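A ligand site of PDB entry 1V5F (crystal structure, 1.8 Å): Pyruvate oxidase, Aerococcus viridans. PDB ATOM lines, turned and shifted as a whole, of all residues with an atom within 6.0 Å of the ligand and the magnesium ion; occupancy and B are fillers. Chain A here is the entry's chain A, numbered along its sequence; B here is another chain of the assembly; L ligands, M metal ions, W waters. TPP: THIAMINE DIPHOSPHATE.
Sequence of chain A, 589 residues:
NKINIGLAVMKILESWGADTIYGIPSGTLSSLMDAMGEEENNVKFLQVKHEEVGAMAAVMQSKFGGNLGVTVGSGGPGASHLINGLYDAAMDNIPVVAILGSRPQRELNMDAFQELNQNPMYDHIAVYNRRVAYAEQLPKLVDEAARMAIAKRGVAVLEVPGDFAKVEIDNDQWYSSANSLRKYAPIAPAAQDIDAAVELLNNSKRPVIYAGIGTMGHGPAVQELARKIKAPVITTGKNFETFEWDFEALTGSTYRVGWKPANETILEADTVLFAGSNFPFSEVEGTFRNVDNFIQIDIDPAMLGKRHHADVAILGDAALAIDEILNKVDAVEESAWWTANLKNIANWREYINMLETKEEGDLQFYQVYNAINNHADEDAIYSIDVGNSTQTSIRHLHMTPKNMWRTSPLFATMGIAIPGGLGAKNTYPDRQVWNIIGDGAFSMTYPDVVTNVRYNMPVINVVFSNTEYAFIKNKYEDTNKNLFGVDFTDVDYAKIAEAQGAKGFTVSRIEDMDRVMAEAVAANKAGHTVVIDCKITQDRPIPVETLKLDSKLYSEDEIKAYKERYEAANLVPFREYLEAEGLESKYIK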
ATOM      1  N   ASN A  84       0.610 -30.057 -21.977  1.00  0.00           N
ATOM      2  CA  ASN A  84       0.481 -29.651 -23.372  1.00  0.00           C
ATOM      3  C   ASN A  84       1.815 -29.528 -24.091  1.00  0.00           C
ATOM      4  O   ASN A  84       1.915 -29.842 -25.275  1.00  0.00           O
ATOM      5  CB  ASN A  84      -0.313 -28.344 -23.498  1.00  0.00           C
ATOM      6  CG  ASN A  84      -1.801 -28.578 -23.372  1.00  0.00           C
ATOM      7  OD1 ASN A  84      -2.260 -29.228 -22.431  1.00  0.00           O
ATOM      8  ND2 ASN A  84      -2.567 -28.059 -24.314  1.00  0.00           N
ATOM      9  N   VAL A 386      -1.852 -21.780 -33.063  1.00  0.00           N
ATOM     10  CA  VAL A 386      -2.880 -22.611 -33.675  1.00  0.00           C
ATOM     11  C   VAL A 386      -4.210 -21.870 -33.784  1.00  0.00           C
ATOM     12  O   VAL A 386      -4.770 -21.431 -32.781  1.00  0.00           O
ATOM     13  CB  VAL A 386      -3.088 -23.911 -32.871  1.00  0.00           C
ATOM     14  CG1 VAL A 386      -4.216 -24.728 -33.485  1.00  0.00           C
ATOM     15  CG2 VAL A 386      -1.801 -24.718 -32.867  1.00  0.00           C
ATOM     16  N   GLY A 387      -4.691 -21.742 -35.005  1.00  0.00           N
ATOM     17  CA  GLY A 387      -5.932 -21.040 -35.253  1.00  0.00           C
ATOM     18  C   GLY A 387      -6.072 -20.768 -36.736  1.00  0.00           C
ATOM     19  O   GLY A 387      -5.138 -21.014 -37.506  1.00  0.00           O
ATOM     20  N   ASN A 388      -7.226 -20.267 -37.146  1.00  0.00           N
ATOM     21  CA  ASN A 388      -7.495 -19.991 -38.546  1.00  0.00           C
ATOM     22  C   ASN A 388      -6.643 -18.830 -39.094  1.00  0.00           C
ATOM     23  O   ASN A 388      -6.018 -18.955 -40.149  1.00  0.00           O
ATOM     24  CB  ASN A 388      -8.981 -19.664 -38.728  1.00  0.00           C
ATOM     25  CG  ASN A 388      -9.458 -19.883 -40.144  1.00  0.00           C
ATOM     26  OD1 ASN A 388     -10.594 -19.568 -40.483  1.00  0.00           O
ATOM     27  ND2 ASN A 388      -8.594 -20.447 -40.982  1.00  0.00           N
ATOM     28  N   SER A 389      -6.635 -17.712 -38.374  1.00  0.00           N
ATOM     29  CA  SER A 389      -5.870 -16.544 -38.810  1.00  0.00           C
ATOM     30  C   SER A 389      -4.367 -16.758 -38.879  1.00  0.00           C
ATOM     31  O   SER A 389      -3.700 -16.254 -39.798  1.00  0.00           O
ATOM     32  CB  SER A 389      -6.173 -15.359 -37.892  1.00  0.00           C
ATOM     33  OG  SER A 389      -7.560 -15.088 -37.830  1.00  0.00           O
ATOM     34  N   THR A 390      -3.821 -17.492 -37.912  1.00  0.00           N
ATOM     35  CA  THR A 390      -2.381 -17.736 -37.860  1.00  0.00           C
ATOM     36  C   THR A 390      -1.888 -18.771 -38.866  1.00  0.00           C
ATOM     37  O   THR A 390      -0.887 -18.548 -39.551  1.00  0.00           O
ATOM     38  CB  THR A 390      -1.952 -18.181 -36.445  1.00  0.00           C
ATOM     39  OG1 THR A 390      -2.748 -19.303 -36.039  1.00  0.00           O
ATOM     40  CG2 THR A 390      -2.148 -17.037 -35.446  1.00  0.00           C
ATOM     41  N   PHE A 411      -0.101 -32.131 -32.675  1.00  0.00           N
ATOM     42  CA  PHE A 411      -0.882 -32.150 -31.441  1.00  0.00           C
ATOM     43  C   PHE A 411      -1.730 -30.886 -31.538  1.00  0.00           C
ATOM     44  O   PHE A 411      -2.840 -30.810 -31.013  1.00  0.00           O
ATOM     45  CB  PHE A 411       0.034 -32.098 -30.211  1.00  0.00           C
ATOM     46  CG  PHE A 411      -0.709 -32.173 -28.897  1.00  0.00           C
ATOM     47  CD1 PHE A 411      -1.527 -33.259 -28.598  1.00  0.00           C
ATOM     48  CD2 PHE A 411      -0.570 -31.159 -27.945  1.00  0.00           C
ATOM     49  CE1 PHE A 411      -2.197 -33.342 -27.382  1.00  0.00           C
ATOM     50  CE2 PHE A 411      -1.233 -31.231 -26.722  1.00  0.00           C
ATOM     51  CZ  PHE A 411      -2.057 -32.329 -26.444  1.00  0.00           C
ATOM     52  N   ALA A 412      -1.185 -29.880 -32.221  1.00  0.00           N
ATOM     53  CA  ALA A 412      -1.860 -28.619 -32.457  1.00  0.00           C
ATOM     54  C   ALA A 412      -2.392 -27.900 -31.229  1.00  0.00           C
ATOM     55  O   ALA A 412      -3.567 -27.515 -31.189  1.00  0.00           O
ATOM     56  CB  ALA A 412      -2.988 -28.837 -33.451  1.00  0.00           C
ATOM     57  N   THR A 413      -1.547 -27.701 -30.225  1.00  0.00           N
ATOM     58  CA  THR A 413      -1.985 -27.007 -29.016  1.00  0.00           C
ATOM     59  C   THR A 413      -1.906 -25.492 -29.157  1.00  0.00           C
ATOM     60  O   THR A 413      -0.902 -24.940 -29.612  1.00  0.00           O
ATOM     61  CB  THR A 413      -1.154 -27.401 -27.773  1.00  0.00           C
ATOM     62  OG1 THR A 413      -1.615 -26.651 -26.645  1.00  0.00           O
ATOM     63  CG2 THR A 413       0.325 -27.111 -27.993  1.00  0.00           C
ATOM     64  N   MET A 414      -2.991 -24.819 -28.785  1.00  0.00           N
ATOM     65  CA  MET A 414      -3.022 -23.368 -28.827  1.00  0.00           C
ATOM     66  C   MET A 414      -2.090 -22.908 -27.709  1.00  0.00           C
ATOM     67  O   MET A 414      -1.870 -23.643 -26.733  1.00  0.00           O
ATOM     68  CB  MET A 414      -4.449 -22.862 -28.568  1.00  0.00           C
ATOM     69  CG  MET A 414      -5.389 -22.974 -29.754  1.00  0.00           C
ATOM     70  SD  MET A 414      -7.118 -22.760 -29.257  1.00  0.00           S
ATOM     71  CE  MET A 414      -7.133 -21.030 -28.784  1.00  0.00           C
ATOM     72  N   GLY A 415      -1.551 -21.704 -27.846  1.00  0.00           N
ATOM     73  CA  GLY A 415      -0.651 -21.160 -26.845  1.00  0.00           C
ATOM     74  C   GLY A 415       0.811 -21.464 -27.117  1.00  0.00           C
ATOM     75  O   GLY A 415       1.674 -21.169 -26.292  1.00  0.00           O
ATOM     76  N   ILE A 437      -0.289 -14.699 -33.385  1.00  0.00           N
ATOM     77  CA  ILE A 437      -1.309 -15.309 -32.532  1.00  0.00           C
ATOM     78  C   ILE A 437      -2.753 -14.860 -32.753  1.00  0.00           C
ATOM     79  O   ILE A 437      -3.008 -13.727 -33.134  1.00  0.00           O
ATOM     80  CB  ILE A 437      -0.974 -14.996 -31.044  1.00  0.00           C
ATOM     81  CG1 ILE A 437       0.538 -14.861 -30.876  1.00  0.00           C
ATOM     82  CG2 ILE A 437      -1.547 -16.066 -30.133  1.00  0.00           C
ATOM     83  CD1 ILE A 437       0.978 -14.285 -29.544  1.00  0.00           C
ATOM     84  N   GLY A 438      -3.695 -15.776 -32.504  1.00  0.00           N
ATOM     85  CA  GLY A 438      -5.098 -15.441 -32.615  1.00  0.00           C
ATOM     86  C   GLY A 438      -5.487 -14.988 -31.221  1.00  0.00           C
ATOM     87  O   GLY A 438      -4.795 -15.351 -30.264  1.00  0.00           O
ATOM     88  N   ASP A 439      -6.555 -14.200 -31.058  1.00  0.00           N
ATOM     89  CA  ASP A 439      -6.915 -13.737 -29.721  1.00  0.00           C
ATOM     90  C   ASP A 439      -7.287 -14.852 -28.749  1.00  0.00           C
ATOM     91  O   ASP A 439      -7.042 -14.735 -27.546  1.00  0.00           O
ATOM     92  CB  ASP A 439      -8.034 -12.670 -29.773  1.00  0.00           C
ATOM     93  CG  ASP A 439      -9.207 -13.087 -30.634  1.00  0.00           C
ATOM     94  OD1 ASP A 439      -9.238 -14.237 -31.078  1.00  0.00           O
ATOM     95  OD2 ASP A 439     -10.109 -12.252 -30.874  1.00  0.00           O
ATOM     96  N   GLY A 440      -7.853 -15.940 -29.267  1.00  0.00           N
ATOM     97  CA  GLY A 440      -8.202 -17.056 -28.400  1.00  0.00           C
ATOM     98  C   GLY A 440      -6.962 -17.697 -27.808  1.00  0.00           C
ATOM     99  O   GLY A 440      -6.904 -17.973 -26.609  1.00  0.00           O
ATOM    100  N   ALA A 441      -5.951 -17.929 -28.641  1.00  0.00           N
ATOM    101  CA  ALA A 441      -4.711 -18.544 -28.177  1.00  0.00           C
ATOM    102  C   ALA A 441      -3.938 -17.551 -27.320  1.00  0.00           C
ATOM    103  O   ALA A 441      -3.302 -17.938 -26.335  1.00  0.00           O
ATOM    104  CB  ALA A 441      -3.865 -18.990 -29.373  1.00  0.00           C
ATOM    105  N   PHE A 442      -3.989 -16.274 -27.688  1.00  0.00           N
ATOM    106  CA  PHE A 442      -3.303 -15.240 -26.933  1.00  0.00           C
ATOM    107  C   PHE A 442      -3.877 -15.210 -25.514  1.00  0.00           C
ATOM    108  O   PHE A 442      -3.134 -15.068 -24.544  1.00  0.00           O
ATOM    109  CB  PHE A 442      -3.511 -13.883 -27.603  1.00  0.00           C
ATOM    110  CG  PHE A 442      -2.657 -12.774 -27.018  1.00  0.00           C
ATOM    111  CD1 PHE A 442      -1.268 -12.865 -27.057  1.00  0.00           C
ATOM    112  CD2 PHE A 442      -3.249 -11.651 -26.470  1.00  0.00           C
ATOM    113  CE1 PHE A 442      -0.479 -11.833 -26.541  1.00  0.00           C
ATOM    114  CE2 PHE A 442      -2.467 -10.610 -25.947  1.00  0.00           C
ATOM    115  CZ  PHE A 442      -1.079 -10.700 -25.986  1.00  0.00           C
ATOM    116  N   MET A 444      -4.860 -17.521 -23.748  1.00  0.00           N
ATOM    117  CA  MET A 444      -4.427 -18.658 -22.939  1.00  0.00           C
ATOM    118  C   MET A 444      -3.000 -18.468 -22.456  1.00  0.00           C
ATOM    119  O   MET A 444      -2.539 -19.200 -21.576  1.00  0.00           O
ATOM    120  CB  MET A 444      -4.472 -19.952 -23.747  1.00  0.00           C
ATOM    121  CG  MET A 444      -5.848 -20.379 -24.214  1.00  0.00           C
ATOM    122  SD  MET A 444      -5.740 -21.919 -25.188  1.00  0.00           S
ATOM    123  CE  MET A 444      -7.508 -22.237 -25.495  1.00  0.00           C
ATOM    124  N   PHE A 464      -4.433 -11.353 -33.715  1.00  0.00           N
ATOM    125  CA  PHE A 464      -5.602 -11.178 -34.567  1.00  0.00           C
ATOM    126  C   PHE A 464      -6.873 -11.213 -33.723  1.00  0.00           C
ATOM    127  O   PHE A 464      -7.290 -12.278 -33.270  1.00  0.00           O
ATOM    128  CB  PHE A 464      -5.664 -12.281 -35.629  1.00  0.00           C
ATOM    129  CG  PHE A 464      -4.556 -12.203 -36.654  1.00  0.00           C
ATOM    130  CD1 PHE A 464      -3.602 -13.216 -36.740  1.00  0.00           C
ATOM    131  CD2 PHE A 464      -4.488 -11.135 -37.537  1.00  0.00           C
ATOM    132  CE1 PHE A 464      -2.587 -13.152 -37.703  1.00  0.00           C
ATOM    133  CE2 PHE A 464      -3.480 -11.062 -38.507  1.00  0.00           C
ATOM    134  CZ  PHE A 464      -2.526 -12.075 -38.580  1.00  0.00           C
ATOM    135  N   SER A 465      -7.470 -10.042 -33.509  1.00  0.00           N
ATOM    136  CA  SER A 465      -8.706  -9.946 -32.725  1.00  0.00           C
ATOM    137  C   SER A 465      -9.904  -9.977 -33.669  1.00  0.00           C
ATOM    138  O   SER A 465     -10.194  -8.986 -34.336  1.00  0.00           O
ATOM    139  CB  SER A 465      -8.718  -8.646 -31.904  1.00  0.00           C
ATOM    140  OG  SER A 465      -7.808  -8.700 -30.827  1.00  0.00           O
ATOM    141  N   ASN A 466     -10.579 -11.106 -33.728  1.00  0.00           N
ATOM    142  CA  ASN A 466     -11.734 -11.252 -34.618  1.00  0.00           C
ATOM    143  C   ASN A 466     -12.957 -11.779 -33.870  1.00  0.00           C
ATOM    144  O   ASN A 466     -13.796 -12.465 -34.455  1.00  0.00           O
ATOM    145  CB  ASN A 466     -11.386 -12.211 -35.770  1.00  0.00           C
ATOM    146  CG  ASN A 466     -11.059 -13.607 -35.280  1.00  0.00           C
ATOM    147  OD1 ASN A 466     -11.121 -13.871 -34.091  1.00  0.00           O
ATOM    148  ND2 ASN A 466     -10.711 -14.498 -36.201  1.00  0.00           N
ATOM    149  N   THR A 467     -13.052 -11.460 -32.580  1.00  0.00           N
ATOM    150  CA  THR A 467     -14.169 -11.887 -31.749  1.00  0.00           C
ATOM    151  C   THR A 467     -14.358 -13.404 -31.780  1.00  0.00           C
ATOM    152  O   THR A 467     -13.690 -14.128 -31.045  1.00  0.00           O
ATOM    153  CB  THR A 467     -15.483 -11.206 -32.188  1.00  0.00           C
ATOM    154  OG1 THR A 467     -15.345  -9.788 -32.041  1.00  0.00           O
ATOM    155  CG2 THR A 467     -16.654 -11.675 -31.342  1.00  0.00           C
ATOM    156  N   ILE B  24     -14.598 -24.453 -23.892  1.00  0.00           N
ATOM    157  CA  ILE B  24     -14.396 -23.618 -25.062  1.00  0.00           C
ATOM    158  C   ILE B  24     -14.925 -24.385 -26.262  1.00  0.00           C
ATOM    159  O   ILE B  24     -14.534 -25.530 -26.502  1.00  0.00           O
ATOM    160  CB  ILE B  24     -12.896 -23.326 -25.289  1.00  0.00           C
ATOM    161  CG1 ILE B  24     -12.331 -22.576 -24.081  1.00  0.00           C
ATOM    162  CG2 ILE B  24     -12.705 -22.525 -26.572  1.00  0.00           C
ATOM    163  CD1 ILE B  24     -10.837 -22.320 -24.158  1.00  0.00           C
ATOM    164  N   PRO B  25     -15.833 -23.779 -27.032  1.00  0.00           N
ATOM    165  CA  PRO B  25     -16.411 -24.448 -28.208  1.00  0.00           C
ATOM    166  C   PRO B  25     -15.435 -24.604 -29.362  1.00  0.00           C
ATOM    167  O   PRO B  25     -14.590 -23.734 -29.597  1.00  0.00           O
ATOM    168  CB  PRO B  25     -17.586 -23.535 -28.568  1.00  0.00           C
ATOM    169  CG  PRO B  25     -17.049 -22.185 -28.229  1.00  0.00           C
ATOM    170  CD  PRO B  25     -16.379 -22.416 -26.887  1.00  0.00           C
ATOM    171  N   SER B  26     -15.536 -25.727 -30.063  1.00  0.00           N
ATOM    172  CA  SER B  26     -14.686 -26.011 -31.222  1.00  0.00           C
ATOM    173  C   SER B  26     -15.190 -27.233 -31.982  1.00  0.00           C
ATOM    174  O   SER B  26     -16.130 -27.902 -31.550  1.00  0.00           O
ATOM    175  CB  SER B  26     -13.226 -26.202 -30.804  1.00  0.00           C
ATOM    176  OG  SER B  26     -13.046 -27.367 -30.027  1.00  0.00           O
ATOM    177  N   GLU B  51      -9.169 -23.909 -20.732  1.00  0.00           N
ATOM    178  CA  GLU B  51      -9.891 -25.094 -20.266  1.00  0.00           C
ATOM    179  C   GLU B  51      -9.635 -25.510 -18.826  1.00  0.00           C
ATOM    180  O   GLU B  51     -10.512 -26.087 -18.184  1.00  0.00           O
ATOM    181  CB  GLU B  51      -9.636 -26.292 -21.192  1.00  0.00           C
ATOM    182  CG  GLU B  51     -10.106 -26.080 -22.615  1.00  0.00           C
ATOM    183  CD  GLU B  51      -9.015 -25.568 -23.527  1.00  0.00           C
ATOM    184  OE1 GLU B  51      -8.072 -24.927 -23.010  1.00  0.00           O
ATOM    185  OE2 GLU B  51      -9.104 -25.796 -24.745  1.00  0.00           O
ATOM    186  N   SER B  74     -11.530 -30.118 -25.978  1.00  0.00           N
ATOM    187  CA  SER B  74     -11.415 -30.599 -27.355  1.00  0.00           C
ATOM    188  C   SER B  74     -10.302 -31.644 -27.522  1.00  0.00           C
ATOM    189  O   SER B  74      -9.347 -31.666 -26.757  1.00  0.00           O
ATOM    190  CB  SER B  74     -11.183 -29.422 -28.309  1.00  0.00           C
ATOM    191  OG  SER B  74     -10.016 -28.703 -27.975  1.00  0.00           O
ATOM    192  N   GLY B  75     -10.452 -32.490 -28.537  1.00  0.00           N
ATOM    193  CA  GLY B  75      -9.472 -33.537 -28.784  1.00  0.00           C
ATOM    194  C   GLY B  75      -8.028 -33.108 -28.677  1.00  0.00           C
ATOM    195  O   GLY B  75      -7.616 -32.140 -29.311  1.00  0.00           O
ATOM    196  N   PRO B  77      -5.113 -31.218 -27.094  1.00  0.00           N
ATOM    197  CA  PRO B  77      -4.774 -30.093 -26.220  1.00  0.00           C
ATOM    198  C   PRO B  77      -5.887 -29.515 -25.351  1.00  0.00           C
ATOM    199  O   PRO B  77      -5.614 -28.920 -24.305  1.00  0.00           O
ATOM    200  CB  PRO B  77      -4.176 -29.074 -27.192  1.00  0.00           C
ATOM    201  CG  PRO B  77      -4.913 -29.356 -28.461  1.00  0.00           C
ATOM    202  CD  PRO B  77      -4.890 -30.870 -28.503  1.00  0.00           C
ATOM    203  N   GLY B  78      -7.126 -29.662 -25.783  1.00  0.00           N
ATOM    204  CA  GLY B  78      -8.234 -29.146 -24.982  1.00  0.00           C
ATOM    205  C   GLY B  78      -8.415 -30.070 -23.794  1.00  0.00           C
ATOM    206  O   GLY B  78      -8.531 -29.628 -22.650  1.00  0.00           O
ATOM    207  N   HIS B  81      -5.656 -29.891 -21.196  1.00  0.00           N
ATOM    208  CA  HIS B  81      -5.698 -28.673 -20.380  1.00  0.00           C
ATOM    209  C   HIS B  81      -6.567 -28.848 -19.143  1.00  0.00           C
ATOM    210  O   HIS B  81      -6.520 -28.042 -18.220  1.00  0.00           O
ATOM    211  CB  HIS B  81      -6.218 -27.492 -21.220  1.00  0.00           C
ATOM    212  CG  HIS B  81      -5.142 -26.617 -21.762  1.00  0.00           C
ATOM    213  ND1 HIS B  81      -5.393 -25.549 -22.601  1.00  0.00           N
ATOM    214  CD2 HIS B  81      -3.797 -26.633 -21.585  1.00  0.00           C
ATOM    215  CE1 HIS B  81      -4.259 -24.953 -22.907  1.00  0.00           C
ATOM    216  NE2 HIS B  81      -3.275 -25.590 -22.304  1.00  0.00           N
ATOM    217  N   GLN B 114      -4.287 -34.236 -35.197  1.00  0.00           N
ATOM    218  CA  GLN B 114      -4.732 -34.108 -33.814  1.00  0.00           C
ATOM    219  C   GLN B 114      -5.543 -35.330 -33.369  1.00  0.00           C
ATOM    220  O   GLN B 114      -6.496 -35.216 -32.595  1.00  0.00           O
ATOM    221  CB  GLN B 114      -5.582 -32.846 -33.685  1.00  0.00           C
ATOM    222  CG  GLN B 114      -5.763 -32.329 -32.276  1.00  0.00           C
ATOM    223  CD  GLN B 114      -6.283 -30.899 -32.260  1.00  0.00           C
ATOM    224  OE1 GLN B 114      -7.365 -30.626 -32.774  1.00  0.00           O
ATOM    225  NE2 GLN B 114      -5.507 -29.996 -31.690  1.00  0.00           N
HETATM  226  N1' TPP L   1      -7.660 -25.854 -26.907  1.00  0.00           N
HETATM  227  C2' TPP L   1      -6.343 -25.989 -27.222  1.00  0.00           C
HETATM  228  CM2 TPP L   1      -5.373 -25.887 -26.106  1.00  0.00           C
HETATM  229  N3' TPP L   1      -5.923 -26.194 -28.461  1.00  0.00           N
HETATM  230  C4' TPP L   1      -6.847 -26.269 -29.484  1.00  0.00           C
HETATM  231  N4' TPP L   1      -6.364 -26.469 -30.687  1.00  0.00           N
HETATM  232  C5' TPP L   1      -8.278 -26.133 -29.186  1.00  0.00           C
HETATM  233  C6' TPP L   1      -8.600 -25.919 -27.889  1.00  0.00           C
HETATM  234  C7' TPP L   1      -9.403 -26.160 -30.186  1.00  0.00           C
HETATM  235  N3  TPP L   1      -9.315 -25.046 -31.205  1.00  0.00           N
HETATM  236  C2  TPP L   1      -8.703 -25.156 -32.373  1.00  0.00           C
HETATM  237  S1  TPP L   1      -8.779 -23.727 -33.264  1.00  0.00           S
HETATM  238  C5  TPP L   1      -9.655 -22.940 -32.029  1.00  0.00           C
HETATM  239  C4  TPP L   1      -9.884 -23.772 -30.973  1.00  0.00           C
HETATM  240  CM4 TPP L   1     -10.616 -23.456 -29.707  1.00  0.00           C
HETATM  241  C6  TPP L   1     -10.059 -21.518 -32.182  1.00  0.00           C
HETATM  242  C7  TPP L   1      -8.949 -20.625 -31.670  1.00  0.00           C
HETATM  243  O7  TPP L   1      -9.333 -19.266 -31.933  1.00  0.00           O
HETATM  244  PA  TPP L   1      -8.261 -18.097 -32.068  1.00  0.00           P
HETATM  245  O1A TPP L   1      -9.024 -16.939 -31.622  1.00  0.00           O
HETATM  246  O2A TPP L   1      -6.932 -18.380 -31.457  1.00  0.00           O
HETATM  247  O3A TPP L   1      -7.978 -18.082 -33.670  1.00  0.00           O
HETATM  248  PB  TPP L   1      -8.832 -17.752 -34.982  1.00  0.00           P
HETATM  249  O1B TPP L   1      -9.369 -19.086 -35.421  1.00  0.00           O
HETATM  250  O2B TPP L   1      -7.948 -17.004 -35.927  1.00  0.00           O
HETATM  251  O3B TPP L   1     -10.012 -16.832 -34.557  1.00  0.00           O
HETATM  252 MG    MG M   1      -9.918 -15.276 -32.887  1.00  0.00          MG
HETATM  253  O   HOH W   1      -5.416 -17.571 -35.394  1.00  0.00           O
HETATM  254  O   HOH W   2      -4.479 -18.637 -32.861  1.00  0.00           O
HETATM  255  O   HOH W   3     -11.963 -16.014 -32.060  1.00  0.00           O
HETATM  256  O   HOH W   4      -7.918 -14.740 -33.984  1.00  0.00           O
HETATM  257  O   HOH W   5      -7.535 -26.251 -35.298  1.00  0.00           O
HETATM  258  O   HOH W   6      -7.135 -27.715 -33.128  1.00  0.00           O
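A nitrogen (N1') of the ligand sits at hydrogen-bond distance from the side-chain carboxylate (OE2) of Glu 51 of chain B (2.6 Å).
N of Ser 389 is in hydrogen-bond range of O2B of the ligand (2.9 Å).
OG of Ser 389 lies within hydrogen-bond range of O2B of the ligand (2.7 Å).
O2A of the ligand lies within hydrogen-bond range of N of Gly 440 (3.4 Å).
The backbone NH of Asn 388 is in hydrogen-bond range of an oxygen (O1B) of the ligand, 3.0 Å away.
N of Ala 441 lies within hydrogen-bond range of O2A of the ligand, at 3.0 Å.
The backbone carbonyl oxygen (O) of Ala 412 is in hydrogen-bond range of a nitrogen (N4') of the ligand, at 3.0 Å.
N of Met 414 is in hydrogen-bond range of N3' of the ligand (3.3 Å).
The magnesium ion is bound by the side-chain carboxylate of Asp 439 (2.2 Å), the side-chain amide oxygen of Asn 466 (2.2 Å), an oxygen (O1A) of the ligand (2.3 Å), an oxygen (O3B) of the ligand (2.3 Å), water W3 (2.3 Å) and water W4 (2.3 Å).
The magnesium ion has six donor atoms within binding distance.
O of Phe 464 sits at hydrogen-bond distance from N of Asp 439.
The side-chain carboxylate (OD2) of Asp 439 is in hydrogen-bond range of the backbone NH (N) of Thr 467 (3.5 Å).
O of Ala 412 is in hydrogen-bond range of NE2 of Gln 114 of chain B (3.2 Å).
O of Pro 77 of chain B sits at hydrogen-bond distance from ND2 of Asn 84, at 3.2 Å.
A ring nitrogen (NE2) of His 81 of chain B lies within hydrogen-bond range of the side-chain amide nitrogen (ND2) of Asn 84 (3.3 Å).
The side-chain amide nitrogen of Gln 114 of chain B is in hydrogen-bond range of the backbone carbonyl oxygen of Phe 411 (2.9 Å).
The side-chain hydroxyl (OG1) of Thr 413 is in hydrogen-bond range of the side-chain amide nitrogen (ND2) of Asn 84 (2.9 Å).
The backbone carbonyl oxygen of Gly 387 sits at hydrogen-bond distance from the side-chain hydroxyl of Thr 390, at 3.3 Å.
Water W4 lies within hydrogen-bond range of O of Phe 464 (2.6 Å), O2B of the ligand (3.0 Å) and N of Asp 439 (3.3 Å).
Water W1 lies within hydrogen-bond range of O2B of the ligand, N of Thr 390 and N of Ser 389.
Water W2 lies within hydrogen-bond range of the backbone carbonyl oxygen of Val 386, an oxygen (O2A) of the ligand and the backbone NH of Gly 438.
Water W6 lies within hydrogen-bond range of N4' of the ligand (2.8 Å) and OE1 of Gln 114 of chain B (2.9 Å).
Two residues have an atom within 4 Å of the magnesium ion: Asp 439 and Asn 466.
The nearest printed residue that does not touch the magnesium ion is Phe 464 (4.01 Å).
ND2 of Asn 84 touches CM2 of the ligand, at 3.98 Å.
Val 386 touches the ligand.
C of Gly 387 touches O1B of the ligand, 3.9 Å away.
OG1 of Thr 413 touches CM2 of the ligand, 3.9 Å away.
Gly 438 touches the ligand (CA to O2A, 3.7 Å).
Met 444 touches the ligand (CE to N1', 3.9 Å).
Ile 24 of chain B touches the ligand.
Pro 25 of chain B touches the ligand.
OG of Ser 26 of chain B touches C7' of the ligand, 3.8 Å away.
Ser 74 of chain B touches the ligand (OG to C6', 3.1 Å).
Pro 77 of chain B touches the ligand (CG to N3', 3.3 Å).
Gly 78 of chain B touches the ligand (CA to N1', 3.9 Å).
His 81 of chain B touches the ligand.
NE2 of Gln 114 of chain B touches N4' of the ligand (3.8 Å).
Hydrophobic or aromatic side chains that line the ligand: Val 386, Met 414, Ala 441, Met 444, Ile 24 of chain B, Pro 77 of chain B and His 81 of chain B.
Of the 32 residues printed, 23 come within 4 Å of the ligand.
Along chain A the residues within 4 Å of the ligand span positions 84 to 466.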
